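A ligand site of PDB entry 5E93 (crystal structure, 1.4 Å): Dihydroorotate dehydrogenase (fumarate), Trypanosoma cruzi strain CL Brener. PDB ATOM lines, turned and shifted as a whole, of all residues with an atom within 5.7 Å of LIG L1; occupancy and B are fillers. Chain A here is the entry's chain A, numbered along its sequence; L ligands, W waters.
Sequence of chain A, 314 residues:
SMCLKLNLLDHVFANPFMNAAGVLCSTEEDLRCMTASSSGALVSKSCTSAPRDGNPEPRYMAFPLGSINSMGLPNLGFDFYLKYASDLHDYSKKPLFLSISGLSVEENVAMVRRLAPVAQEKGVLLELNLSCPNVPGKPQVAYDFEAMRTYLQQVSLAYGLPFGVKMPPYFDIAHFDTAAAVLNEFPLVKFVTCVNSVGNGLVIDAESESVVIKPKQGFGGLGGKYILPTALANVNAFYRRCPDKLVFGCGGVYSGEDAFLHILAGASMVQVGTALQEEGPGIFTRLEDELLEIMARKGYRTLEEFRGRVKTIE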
ATOM      1  N   ALA A  20     -20.980   0.062  20.970  1.00  0.00           N
ATOM      2  CA  ALA A  20     -21.258   0.491  22.310  1.00  0.00           C
ATOM      3  C   ALA A  20     -21.557   1.938  22.327  1.00  0.00           C
ATOM      4  O   ALA A  20     -20.926   2.733  21.631  1.00  0.00           O
ATOM      5  CB  ALA A  20     -20.070   0.166  23.183  1.00  0.00           C
ATOM      6  N   ALA A  21     -22.506   2.389  23.180  1.00  0.00           N
ATOM      7  CA  ALA A  21     -22.804   3.807  23.256  1.00  0.00           C
ATOM      8  C   ALA A  21     -21.580   4.610  23.535  1.00  0.00           C
ATOM      9  O   ALA A  21     -20.678   4.235  24.315  1.00  0.00           O
ATOM     10  CB  ALA A  21     -23.827   4.060  24.309  1.00  0.00           C
ATOM     11  N   GLY A  22     -21.461   5.754  22.900  1.00  0.00           N
ATOM     12  CA  GLY A  22     -20.319   6.639  22.985  1.00  0.00           C
ATOM     13  C   GLY A  22     -19.282   6.475  21.910  1.00  0.00           C
ATOM     14  O   GLY A  22     -18.510   7.375  21.672  1.00  0.00           O
ATOM     15  N   VAL A  23     -19.217   5.298  21.273  1.00  0.00           N
ATOM     16  CA  VAL A  23     -18.200   5.027  20.251  1.00  0.00           C
ATOM     17  C   VAL A  23     -18.846   5.113  18.855  1.00  0.00           C
ATOM     18  O   VAL A  23     -19.856   4.461  18.599  1.00  0.00           O
ATOM     19  CB  VAL A  23     -17.554   3.648  20.501  1.00  0.00           C
ATOM     20  CG1 VAL A  23     -16.554   3.329  19.392  1.00  0.00           C
ATOM     21  CG2 VAL A  23     -16.816   3.619  21.878  1.00  0.00           C
ATOM     22  N   LYS A  45     -24.866   8.233  21.025  1.00  0.00           N
ATOM     23  CA  LYS A  45     -24.115   8.721  22.186  1.00  0.00           C
ATOM     24  C   LYS A  45     -25.043   9.149  23.324  1.00  0.00           C
ATOM     25  O   LYS A  45     -26.056   9.842  23.043  1.00  0.00           O
ATOM     26  CB  LYS A  45     -23.319   9.960  21.697  1.00  0.00           C
ATOM     27  CG  LYS A  45     -22.716  10.844  22.797  1.00  0.00           C
ATOM     28  CD  LYS A  45     -21.635  10.103  23.480  1.00  0.00           C
ATOM     29  CE  LYS A  45     -21.169  10.881  24.766  1.00  0.00           C
ATOM     30  NZ  LYS A  45     -20.097   9.958  25.456  1.00  0.00           N
ATOM     31  N   SER A  46     -24.701   8.805  24.546  1.00  0.00           N
ATOM     32  CA  SER A  46     -25.550   9.260  25.693  1.00  0.00           C
ATOM     33  C   SER A  46     -25.673  10.777  25.668  1.00  0.00           C
ATOM     34  O   SER A  46     -24.694  11.514  25.530  1.00  0.00           O
ATOM     35  CB  SER A  46     -24.986   8.858  27.062  1.00  0.00           C
ATOM     36  OG  SER A  46     -25.052   7.442  27.150  1.00  0.00           O
ATOM     37  N   TYR A  60      -9.349  10.404  26.181  1.00  0.00           N
ATOM     38  CA  TYR A  60      -9.429   8.998  25.774  1.00  0.00           C
ATOM     39  C   TYR A  60      -8.056   8.589  25.382  1.00  0.00           C
ATOM     40  O   TYR A  60      -7.422   9.295  24.576  1.00  0.00           O
ATOM     41  CB  TYR A  60     -10.375   8.785  24.597  1.00  0.00           C
ATOM     42  CG  TYR A  60     -10.325   7.384  23.992  1.00  0.00           C
ATOM     43  CD1 TYR A  60     -11.043   6.353  24.461  1.00  0.00           C
ATOM     44  CD2 TYR A  60      -9.467   7.103  22.872  1.00  0.00           C
ATOM     45  CE1 TYR A  60     -10.961   5.074  23.942  1.00  0.00           C
ATOM     46  CE2 TYR A  60      -9.321   5.847  22.380  1.00  0.00           C
ATOM     47  CZ  TYR A  60     -10.080   4.821  22.863  1.00  0.00           C
ATOM     48  OH  TYR A  60     -10.013   3.530  22.365  1.00  0.00           O
ATOM     49  N   SER A  67      -8.561   0.498  26.953  1.00  0.00           N
ATOM     50  CA  SER A  67      -8.650   1.941  26.905  1.00  0.00           C
ATOM     51  C   SER A  67      -9.033   2.491  28.251  1.00  0.00           C
ATOM     52  O   SER A  67      -9.552   1.802  29.122  1.00  0.00           O
ATOM     53  CB  SER A  67      -9.658   2.401  25.862  1.00  0.00           C
ATOM     54  OG  SER A  67     -11.009   2.039  26.224  1.00  0.00           O
ATOM     55  N   ASN A  69     -10.902   6.274  29.641  1.00  0.00           N
ATOM     56  CA  ASN A  69     -11.563   7.491  29.161  1.00  0.00           C
ATOM     57  C   ASN A  69     -12.255   8.250  30.283  1.00  0.00           C
ATOM     58  O   ASN A  69     -12.815   7.653  31.194  1.00  0.00           O
ATOM     59  CB  ASN A  69     -12.615   7.231  28.029  1.00  0.00           C
ATOM     60  CG  ASN A  69     -14.012   6.888  28.514  1.00  0.00           C
ATOM     61  OD1 ASN A  69     -14.780   7.812  28.865  1.00  0.00           O
ATOM     62  ND2 ASN A  69     -14.366   5.643  28.624  1.00  0.00           N
ATOM     63  N   MET A  71     -14.569  10.914  29.180  1.00  0.00           N
ATOM     64  CA  MET A  71     -15.210  11.823  28.222  1.00  0.00           C
ATOM     65  C   MET A  71     -16.103  12.886  28.878  1.00  0.00           C
ATOM     66  O   MET A  71     -16.035  14.027  28.445  1.00  0.00           O
ATOM     67  CB  MET A  71     -15.974  11.020  27.162  1.00  0.00           C
ATOM     68  CG  MET A  71     -15.284  10.025  26.330  1.00  0.00           C
ATOM     69  SD  MET A  71     -13.881  10.680  25.423  1.00  0.00           S
ATOM     70  CE  MET A  71     -14.783  11.596  24.225  1.00  0.00           C
ATOM     71  N   SER A  99     -29.510   6.477  23.497  1.00  0.00           N
ATOM     72  CA  SER A  99     -29.026   6.455  24.894  1.00  0.00           C
ATOM     73  C   SER A  99     -29.231   7.798  25.543  1.00  0.00           C
ATOM     74  O   SER A  99     -28.878   8.818  24.945  1.00  0.00           O
ATOM     75  CB  SER A  99     -27.577   6.066  24.989  1.00  0.00           C
ATOM     76  OG  SER A  99     -27.136   6.126  26.323  1.00  0.00           O
ATOM     77  N   GLU A 127     -32.202   3.263  25.605  1.00  0.00           N
ATOM     78  CA  GLU A 127     -31.205   2.738  26.545  1.00  0.00           C
ATOM     79  C   GLU A 127     -30.949   3.810  27.553  1.00  0.00           C
ATOM     80  O   GLU A 127     -30.354   4.852  27.268  1.00  0.00           O
ATOM     81  CB  GLU A 127     -29.940   2.232  25.843  1.00  0.00           C
ATOM     82  CG  GLU A 127     -28.930   1.513  26.787  1.00  0.00           C
ATOM     83  CD  GLU A 127     -27.710   0.940  26.054  1.00  0.00           C
ATOM     84  OE1 GLU A 127     -26.705   1.691  25.847  1.00  0.00           O
ATOM     85  OE2 GLU A 127     -27.610  -0.233  25.659  1.00  0.00           O
ATOM     86  N   ASN A 129     -28.996   5.231  30.526  1.00  0.00           N
ATOM     87  CA  ASN A 129     -27.666   5.046  31.084  1.00  0.00           C
ATOM     88  C   ASN A 129     -27.643   5.383  32.590  1.00  0.00           C
ATOM     89  O   ASN A 129     -27.738   6.555  32.932  1.00  0.00           O
ATOM     90  CB  ASN A 129     -26.697   5.932  30.292  1.00  0.00           C
ATOM     91  CG  ASN A 129     -25.244   5.767  30.716  1.00  0.00           C
ATOM     92  OD1 ASN A 129     -24.934   5.000  31.678  1.00  0.00           O
ATOM     93  ND2 ASN A 129     -24.365   6.455  30.048  1.00  0.00           N
ATOM     94  N   SER A 131     -24.995   4.444  34.527  1.00  0.00           N
ATOM     95  CA  SER A 131     -23.652   4.070  34.864  1.00  0.00           C
ATOM     96  C   SER A 131     -22.440   4.850  34.440  1.00  0.00           C
ATOM     97  O   SER A 131     -21.347   4.375  34.489  1.00  0.00           O
ATOM     98  CB  SER A 131     -23.444   2.641  34.374  1.00  0.00           C
ATOM     99  OG  SER A 131     -23.912   2.419  33.093  1.00  0.00           O
ATOM    100  N   LYS A 166     -28.410   0.647  30.806  1.00  0.00           N
ATOM    101  CA  LYS A 166     -26.942   0.440  30.740  1.00  0.00           C
ATOM    102  C   LYS A 166     -26.388   0.403  32.126  1.00  0.00           C
ATOM    103  O   LYS A 166     -26.480   1.406  32.867  1.00  0.00           O
ATOM    104  CB  LYS A 166     -26.305   1.523  29.930  1.00  0.00           C
ATOM    105  CG  LYS A 166     -24.761   1.401  29.757  1.00  0.00           C
ATOM    106  CD  LYS A 166     -24.414   0.251  28.817  1.00  0.00           C
ATOM    107  CE  LYS A 166     -22.941   0.272  28.364  1.00  0.00           C
ATOM    108  NZ  LYS A 166     -22.603   1.399  27.453  1.00  0.00           N
ATOM    109  N   VAL A 195     -21.601  -4.497  30.193  1.00  0.00           N
ATOM    110  CA  VAL A 195     -21.402  -3.435  31.177  1.00  0.00           C
ATOM    111  C   VAL A 195     -20.942  -2.143  30.531  1.00  0.00           C
ATOM    112  O   VAL A 195     -20.314  -2.144  29.461  1.00  0.00           O
ATOM    113  CB  VAL A 195     -20.414  -3.891  32.257  1.00  0.00           C
ATOM    114  CG1 VAL A 195     -20.996  -5.069  33.074  1.00  0.00           C
ATOM    115  CG2 VAL A 195     -19.059  -4.218  31.723  1.00  0.00           C
ATOM    116  N   ASN A 196     -21.133  -1.060  31.257  1.00  0.00           N
ATOM    117  CA  ASN A 196     -20.364   0.166  31.074  1.00  0.00           C
ATOM    118  C   ASN A 196     -18.953  -0.060  31.508  1.00  0.00           C
ATOM    119  O   ASN A 196     -18.566  -1.124  32.018  1.00  0.00           O
ATOM    120  CB  ASN A 196     -21.076   1.298  31.842  1.00  0.00           C
ATOM    121  CG  ASN A 196     -20.935   2.660  31.184  1.00  0.00           C
ATOM    122  OD1 ASN A 196     -19.871   2.991  30.645  1.00  0.00           O
ATOM    123  ND2 ASN A 196     -21.968   3.472  31.190  1.00  0.00           N
ATOM    124  N   SER A 197     -18.116   0.962  31.301  1.00  0.00           N
ATOM    125  CA  SER A 197     -16.697   0.912  31.715  1.00  0.00           C
ATOM    126  C   SER A 197     -16.485   0.603  33.102  1.00  0.00           C
ATOM    127  O   SER A 197     -17.321   0.937  33.985  1.00  0.00           O
ATOM    128  CB  SER A 197     -16.163   2.309  31.682  1.00  0.00           C
ATOM    129  OG  SER A 197     -16.230   2.735  30.394  1.00  0.00           O
ATOM    130  N   LEU A 222     -12.404   2.125  32.356  1.00  0.00           N
ATOM    131  CA  LEU A 222     -11.627   1.138  31.595  1.00  0.00           C
ATOM    132  C   LEU A 222     -12.500   0.334  30.662  1.00  0.00           C
ATOM    133  O   LEU A 222     -13.541  -0.153  31.036  1.00  0.00           O
ATOM    134  CB  LEU A 222     -10.866   0.205  32.521  1.00  0.00           C
ATOM    135  CG  LEU A 222      -9.998   0.851  33.543  1.00  0.00           C
ATOM    136  CD1 LEU A 222      -9.513  -0.187  34.529  1.00  0.00           C
ATOM    137  CD2 LEU A 222      -8.821   1.572  32.899  1.00  0.00           C
ATOM    138  N   GLY A 223     -11.990   0.110  29.475  1.00  0.00           N
ATOM    139  CA  GLY A 223     -12.583  -0.794  28.483  1.00  0.00           C
ATOM    140  C   GLY A 223     -11.582  -1.683  27.850  1.00  0.00           C
ATOM    141  O   GLY A 223     -10.357  -1.494  28.086  1.00  0.00           O
ATOM    142  N   GLY A 224     -12.057  -2.652  27.066  1.00  0.00           N
ATOM    143  CA  GLY A 224     -11.158  -3.487  26.306  1.00  0.00           C
ATOM    144  C   GLY A 224     -10.725  -4.759  26.993  1.00  0.00           C
ATOM    145  O   GLY A 224     -11.507  -5.334  27.802  1.00  0.00           O
ATOM    146  N   LYS A 225      -9.543  -5.227  26.669  1.00  0.00           N
ATOM    147  CA  LYS A 225      -9.115  -6.570  27.187  1.00  0.00           C
ATOM    148  C   LYS A 225      -9.110  -6.638  28.710  1.00  0.00           C
ATOM    149  O   LYS A 225      -9.337  -7.728  29.242  1.00  0.00           O
ATOM    150  CB  LYS A 225      -7.754  -6.966  26.643  1.00  0.00           C
ATOM    151  CG  LYS A 225      -7.645  -6.794  25.135  1.00  0.00           C
ATOM    152  CD  LYS A 225      -7.257  -7.991  24.419  1.00  0.00           C
ATOM    153  CE  LYS A 225      -7.126  -7.684  22.922  1.00  0.00           C
ATOM    154  NZ  LYS A 225      -7.665  -8.920  22.198  1.00  0.00           N
ATOM    155  N   ILE A 227     -11.241  -5.854  30.733  1.00  0.00           N
ATOM    156  CA  ILE A 227     -12.534  -5.974  31.336  1.00  0.00           C
ATOM    157  C   ILE A 227     -13.348  -7.202  30.893  1.00  0.00           C
ATOM    158  O   ILE A 227     -14.461  -7.377  31.391  1.00  0.00           O
ATOM    159  CB  ILE A 227     -13.402  -4.687  31.285  1.00  0.00           C
ATOM    160  CG1 ILE A 227     -14.109  -4.491  29.944  1.00  0.00           C
ATOM    161  CG2 ILE A 227     -12.573  -3.463  31.745  1.00  0.00           C
ATOM    162  CD1 ILE A 227     -15.195  -3.470  30.034  1.00  0.00           C
ATOM    163  N   CYS A 250     -21.582  -6.175  26.723  1.00  0.00           N
ATOM    164  CA  CYS A 250     -20.644  -5.150  26.289  1.00  0.00           C
ATOM    165  C   CYS A 250     -19.405  -5.285  27.150  1.00  0.00           C
ATOM    166  O   CYS A 250     -19.549  -5.363  28.391  1.00  0.00           O
ATOM    167  CB  CYS A 250     -21.272  -3.775  26.446  1.00  0.00           C
ATOM    168  SG  CYS A 250     -20.289  -2.435  25.780  1.00  0.00           S
ATOM    169  N   GLY A 251     -18.240  -5.318  26.569  1.00  0.00           N
ATOM    170  CA  GLY A 251     -16.994  -5.242  27.365  1.00  0.00           C
ATOM    171  C   GLY A 251     -16.013  -6.243  26.802  1.00  0.00           C
ATOM    172  O   GLY A 251     -16.249  -7.473  26.817  1.00  0.00           O
ATOM    173  N   GLY A 252     -14.892  -5.774  26.281  1.00  0.00           N
ATOM    174  CA  GLY A 252     -13.840  -6.644  25.929  1.00  0.00           C
ATOM    175  C   GLY A 252     -13.995  -7.409  24.644  1.00  0.00           C
ATOM    176  O   GLY A 252     -13.238  -8.378  24.420  1.00  0.00           O
ATOM    177  N   VAL A 253     -14.900  -7.026  23.752  1.00  0.00           N
ATOM    178  CA  VAL A 253     -15.061  -7.786  22.504  1.00  0.00           C
ATOM    179  C   VAL A 253     -14.124  -7.254  21.409  1.00  0.00           C
ATOM    180  O   VAL A 253     -14.239  -6.106  20.994  1.00  0.00           O
ATOM    181  CB  VAL A 253     -16.503  -7.687  22.000  1.00  0.00           C
ATOM    182  CG1 VAL A 253     -16.659  -8.385  20.641  1.00  0.00           C
ATOM    183  CG2 VAL A 253     -17.470  -8.294  23.020  1.00  0.00           C
ATOM    184  N   GLN A 271     -22.249  -5.650  22.069  1.00  0.00           N
ATOM    185  CA  GLN A 271     -21.815  -4.281  21.737  1.00  0.00           C
ATOM    186  C   GLN A 271     -20.286  -4.227  21.775  1.00  0.00           C
ATOM    187  O   GLN A 271     -19.621  -4.955  22.519  1.00  0.00           O
ATOM    188  CB  GLN A 271     -22.353  -3.312  22.737  1.00  0.00           C
ATOM    189  CG  GLN A 271     -23.874  -3.456  23.027  1.00  0.00           C
ATOM    190  CD  GLN A 271     -24.417  -2.289  23.775  1.00  0.00           C
ATOM    191  OE1 GLN A 271     -23.691  -1.676  24.562  1.00  0.00           O
ATOM    192  NE2 GLN A 271     -25.664  -1.973  23.605  1.00  0.00           N
ATOM    193  N   VAL A 272     -19.708  -3.368  20.923  1.00  0.00           N
ATOM    194  CA  VAL A 272     -18.234  -3.203  20.709  1.00  0.00           C
ATOM    195  C   VAL A 272     -17.863  -1.760  20.892  1.00  0.00           C
ATOM    196  O   VAL A 272     -18.343  -0.881  20.171  1.00  0.00           O
ATOM    197  CB  VAL A 272     -17.930  -3.716  19.297  1.00  0.00           C
ATOM    198  CG1 VAL A 272     -16.457  -3.767  19.112  1.00  0.00           C
ATOM    199  CG2 VAL A 272     -18.564  -5.080  19.020  1.00  0.00           C
ATOM    200  N   GLY A 273     -17.013  -1.506  21.909  1.00  0.00           N
ATOM    201  CA  GLY A 273     -16.590  -0.171  22.221  1.00  0.00           C
ATOM    202  C   GLY A 273     -15.157   0.055  21.791  1.00  0.00           C
ATOM    203  O   GLY A 273     -14.852   0.440  20.662  1.00  0.00           O
ATOM    204  N   THR A 274     -14.242  -0.173  22.717  1.00  0.00           N
ATOM    205  CA  THR A 274     -12.790   0.040  22.491  1.00  0.00           C
ATOM    206  C   THR A 274     -12.322  -0.520  21.146  1.00  0.00           C
ATOM    207  O   THR A 274     -11.593   0.149  20.407  1.00  0.00           O
ATOM    208  CB  THR A 274     -11.998  -0.549  23.694  1.00  0.00           C
ATOM    209  OG1 THR A 274     -12.342   0.138  24.874  1.00  0.00           O
ATOM    210  CG2 THR A 274     -10.469  -0.388  23.419  1.00  0.00           C
ATOM    211  N   ALA A 275     -12.665  -1.784  20.873  1.00  0.00           N
ATOM    212  CA  ALA A 275     -12.129  -2.395  19.693  1.00  0.00           C
ATOM    213  C   ALA A 275     -12.632  -1.690  18.425  1.00  0.00           C
ATOM    214  O   ALA A 275     -11.888  -1.594  17.404  1.00  0.00           O
ATOM    215  CB  ALA A 275     -12.419  -3.862  19.633  1.00  0.00           C
ATOM    216  N   GLN A 277     -13.532   1.603  18.403  1.00  0.00           N
ATOM    217  CA  GLN A 277     -12.815   2.871  18.372  1.00  0.00           C
ATOM    218  C   GLN A 277     -11.446   2.719  17.765  1.00  0.00           C
ATOM    219  O   GLN A 277     -10.979   3.594  17.002  1.00  0.00           O
ATOM    220  CB  GLN A 277     -12.729   3.395  19.807  1.00  0.00           C
ATOM    221  CG  GLN A 277     -11.944   4.729  19.907  1.00  0.00           C
ATOM    222  CD  GLN A 277     -12.563   5.873  19.173  1.00  0.00           C
ATOM    223  OE1 GLN A 277     -11.791   6.738  18.695  1.00  0.00           O
ATOM    224  NE2 GLN A 277     -13.844   5.943  19.144  1.00  0.00           N
HETATM  225  N1  LIG L   1     -21.231   4.241  27.603  1.00  0.00           N
HETATM  226  C1  LIG L   1     -22.458   4.843  27.574  1.00  0.00           C
HETATM  227  O1  LIG L   1     -23.421   4.172  27.999  1.00  0.00           O
HETATM  228  N2  LIG L   1     -22.610   6.092  27.064  1.00  0.00           N
HETATM  229  C2  LIG L   1     -21.627   6.862  26.590  1.00  0.00           C
HETATM  230  O2  LIG L   1     -21.872   7.977  26.070  1.00  0.00           O
HETATM  231  C3  LIG L   1     -20.350   6.299  26.609  1.00  0.00           C
HETATM  232  N3  LIG L   1     -19.319   6.983  26.085  1.00  0.00           N
HETATM  233  C4  LIG L   1     -18.114   6.302  25.872  1.00  0.00           C
HETATM  234  C5  LIG L   1     -17.066   6.904  25.205  1.00  0.00           C
HETATM  235  C6  LIG L   1     -15.884   6.264  24.907  1.00  0.00           C
HETATM  236  C7  LIG L   1     -14.795   6.960  24.153  1.00  0.00           C
HETATM  237  C8  LIG L   1     -15.692   4.916  25.365  1.00  0.00           C
HETATM  238  C9  LIG L   1     -14.402   4.165  25.164  1.00  0.00           C
HETATM  239  C10 LIG L   1     -16.724   4.339  26.067  1.00  0.00           C
HETATM  240  C11 LIG L   1     -17.949   4.960  26.343  1.00  0.00           C
HETATM  241  N4  LIG L   1     -18.997   4.340  27.018  1.00  0.00           N
HETATM  242  C12 LIG L   1     -20.213   4.960  27.111  1.00  0.00           C
HETATM  243  C13 LIG L   1     -18.826   2.977  27.490  1.00  0.00           C
HETATM  244  C14 LIG L   1     -18.934   1.940  26.409  1.00  0.00           C
HETATM  245  O3  LIG L   1     -20.286   1.973  25.877  1.00  0.00           O
HETATM  246  C15 LIG L   1     -18.693   0.514  26.860  1.00  0.00           C
HETATM  247  O4  LIG L   1     -19.658   0.238  27.894  1.00  0.00           O
HETATM  248  C16 LIG L   1     -17.272   0.349  27.414  1.00  0.00           C
HETATM  249  O5  LIG L   1     -16.354   1.030  26.626  1.00  0.00           O
HETATM  250  C17 LIG L   1     -16.862  -1.078  27.576  1.00  0.00           C
HETATM  251  O6  LIG L   1     -16.923  -1.792  26.335  1.00  0.00           O
HETATM  252  P1  LIG L   1     -15.475  -2.104  25.577  1.00  0.00           P
HETATM  253  O7  LIG L   1     -14.681  -3.028  26.445  1.00  0.00           O
HETATM  254  O8  LIG L   1     -14.825  -0.752  25.384  1.00  0.00           O
HETATM  255  O9  LIG L   1     -15.933  -2.710  24.258  1.00  0.00           O
HETATM  256  C1  LG2 L   2     -18.350   8.154  29.866  1.00  0.00           C
HETATM  257  C2  LG2 L   2     -19.695   8.001  30.133  1.00  0.00           C
HETATM  258  C3  LG2 L   2     -20.116   6.600  30.179  1.00  0.00           C
HETATM  259  N1  LG2 L   2     -19.222   5.641  30.031  1.00  0.00           N
HETATM  260  N2  LG2 L   2     -17.548   7.133  29.517  1.00  0.00           N
HETATM  261  C4  LG2 L   2     -22.496  12.678  28.740  1.00  0.00           C
HETATM  262  C5  LG2 L   2     -23.743  13.096  28.274  1.00  0.00           C
HETATM  263  C6  LG2 L   2     -24.600  12.068  28.569  1.00  0.00           C
HETATM  264  O1  LG2 L   2     -23.927  10.988  29.168  1.00  0.00           O
HETATM  265  C7  LG2 L   2     -22.708  11.379  29.136  1.00  0.00           C
HETATM  266  C8  LG2 L   2     -21.680  10.664  29.725  1.00  0.00           C
HETATM  267  C9  LG2 L   2     -21.770   9.439  30.140  1.00  0.00           C
HETATM  268  C10 LG2 L   2     -20.456   9.173  30.686  1.00  0.00           C
HETATM  269  O2  LG2 L   2     -17.839   9.379  29.837  1.00  0.00           O
HETATM  270  C11 LG2 L   2     -17.985   5.877  29.680  1.00  0.00           C
HETATM  271  O3  LG2 L   2     -17.095   5.030  29.615  1.00  0.00           O
HETATM  272  O4  LG2 L   2     -21.322   6.311  30.406  1.00  0.00           O
HETATM  273  O   HOH W   1     -17.185  -5.045  23.946  1.00  0.00           O
HETATM  274  O   HOH W   2     -14.648   2.086  28.440  1.00  0.00           O
HETATM  275  O   HOH W   3     -17.979   9.696  23.307  1.00  0.00           O
HETATM  276  O   HOH W   4     -26.172   3.935  27.324  1.00  0.00           O
HETATM  277  O   HOH W   5     -13.964  -3.640  22.562  1.00  0.00           O
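The backbone NH (N) of Thr 274 sits at hydrogen-bond distance from an oxygen (O8) of LIG L1. O8 of LIG L1 lies within hydrogen-bond range of OG1 of Thr 274. The backbone NH of Gly 224 is in hydrogen-bond range of an oxygen (O7) of LIG L1, at 2.7 Å. NZ of Lys 45 is in hydrogen-bond range of O2 of LIG L1, at 2.7 Å. N of Gly 252 lies within hydrogen-bond range of O7 of LIG L1 (2.8 Å). O3 of LIG L1 sits at hydrogen-bond distance from O of Ala 21 (2.8 Å). N of Ser 46 lies within hydrogen-bond range of O2 of LIG L1, at 3.3 Å. OG of Ser 46 sits at hydrogen-bond distance from N2 of LIG L1. O9 of LIG L1 sits at hydrogen-bond distance from N of Gly 273, 2.9 Å away. The side-chain amino group (NZ) of Lys 166 sits at hydrogen-bond distance from an oxygen (O3) of LIG L1 (2.9 Å). O of Val 195 is in hydrogen-bond range of O4 of LIG L1 (2.9 Å). ND2 of Asn 129 sits at hydrogen-bond distance from O1 of LIG L1, at 3.2 Å. SG of Cys 250 sits at hydrogen-bond distance from O4 of LIG L1 (3.5 Å). O4 of LG2 L2 sits at hydrogen-bond distance from ND2 of Asn 129 (3.1 Å). OD1 of Asn 196 lies within hydrogen-bond range of N1 of LG2 L2, 2.8 Å away. OD1 of Asn 69 is in hydrogen-bond range of N2 of LG2 L2, at 2.9 Å. The side-chain hydroxyl (OG) of Ser 197 sits at hydrogen-bond distance from an oxygen (O3) of LG2 L2, at 2.6 Å.
A nitrogen (N1) of LIG L1 lies close to a nitrogen (N1) of LG2 L2, at 3.4 Å.
The side-chain hydroxyl of Thr 274 lies within hydrogen-bond range of the side-chain hydroxyl of Ser 67 (2.7 Å). The side-chain hydroxyl (OG) of Ser 99 lies within hydrogen-bond range of the side-chain hydroxyl (OG) of Ser 46 (2.6 Å). O of Lys 166 lies within hydrogen-bond range of OG of Ser 131. ND2 of Asn 196 sits at hydrogen-bond distance from OD1 of Asn 129 (3.4 Å). The backbone NH (N) of Ala 20 sits at hydrogen-bond distance from the backbone carbonyl oxygen (O) of Val 272 (2.9 Å). The side-chain sulfur (SG) of Cys 250 sits at hydrogen-bond distance from the side-chain amide oxygen (OE1) of Gln 271 (3.7 Å). The backbone NH (N) of Met 71 is in hydrogen-bond range of the side-chain amide oxygen (OD1) of Asn 69, at 3.1 Å. N of Ser 67 sits at hydrogen-bond distance from O of Gly 223 (2.9 Å).
Merely in contact with LIG L1: Ala 20, Asn 196, Gly 22, Gly 251, Asn 69, Ile 227, Gly 223, Tyr 60, Met 71, Ser 197, Val 23 and Val 272. Hydrophobic or aromatic side chains that line LIG L1: Ala 20, Ala 21, Val 23, Tyr 60, Met 71 and Ile 227. Along chain A the residues within 4 Å of LIG L1 span positions 20 to 274.
Water W2 lies within hydrogen-bond range of the side-chain hydroxyl of Ser 197 (2.6 Å), an oxygen (O5) of LIG L1 (2.7 Å) and the backbone NH of Gly 223 (3.5 Å). Water W5 lies within hydrogen-bond range of O9 of LIG L1 (2.8 Å), N of Ala 275 (2.8 Å), O of Val 253 (2.9 Å) and N of Thr 274 (3.5 Å). Water W4 lies within hydrogen-bond range of OG of Ser 99, OE1 of Glu 127 and O1 of LIG L1. Water W3 lies within hydrogen-bond range of the backbone carbonyl oxygen of Gly 22 (2.9 Å) and the side-chain amino group of Lys 45 (3.0 Å).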
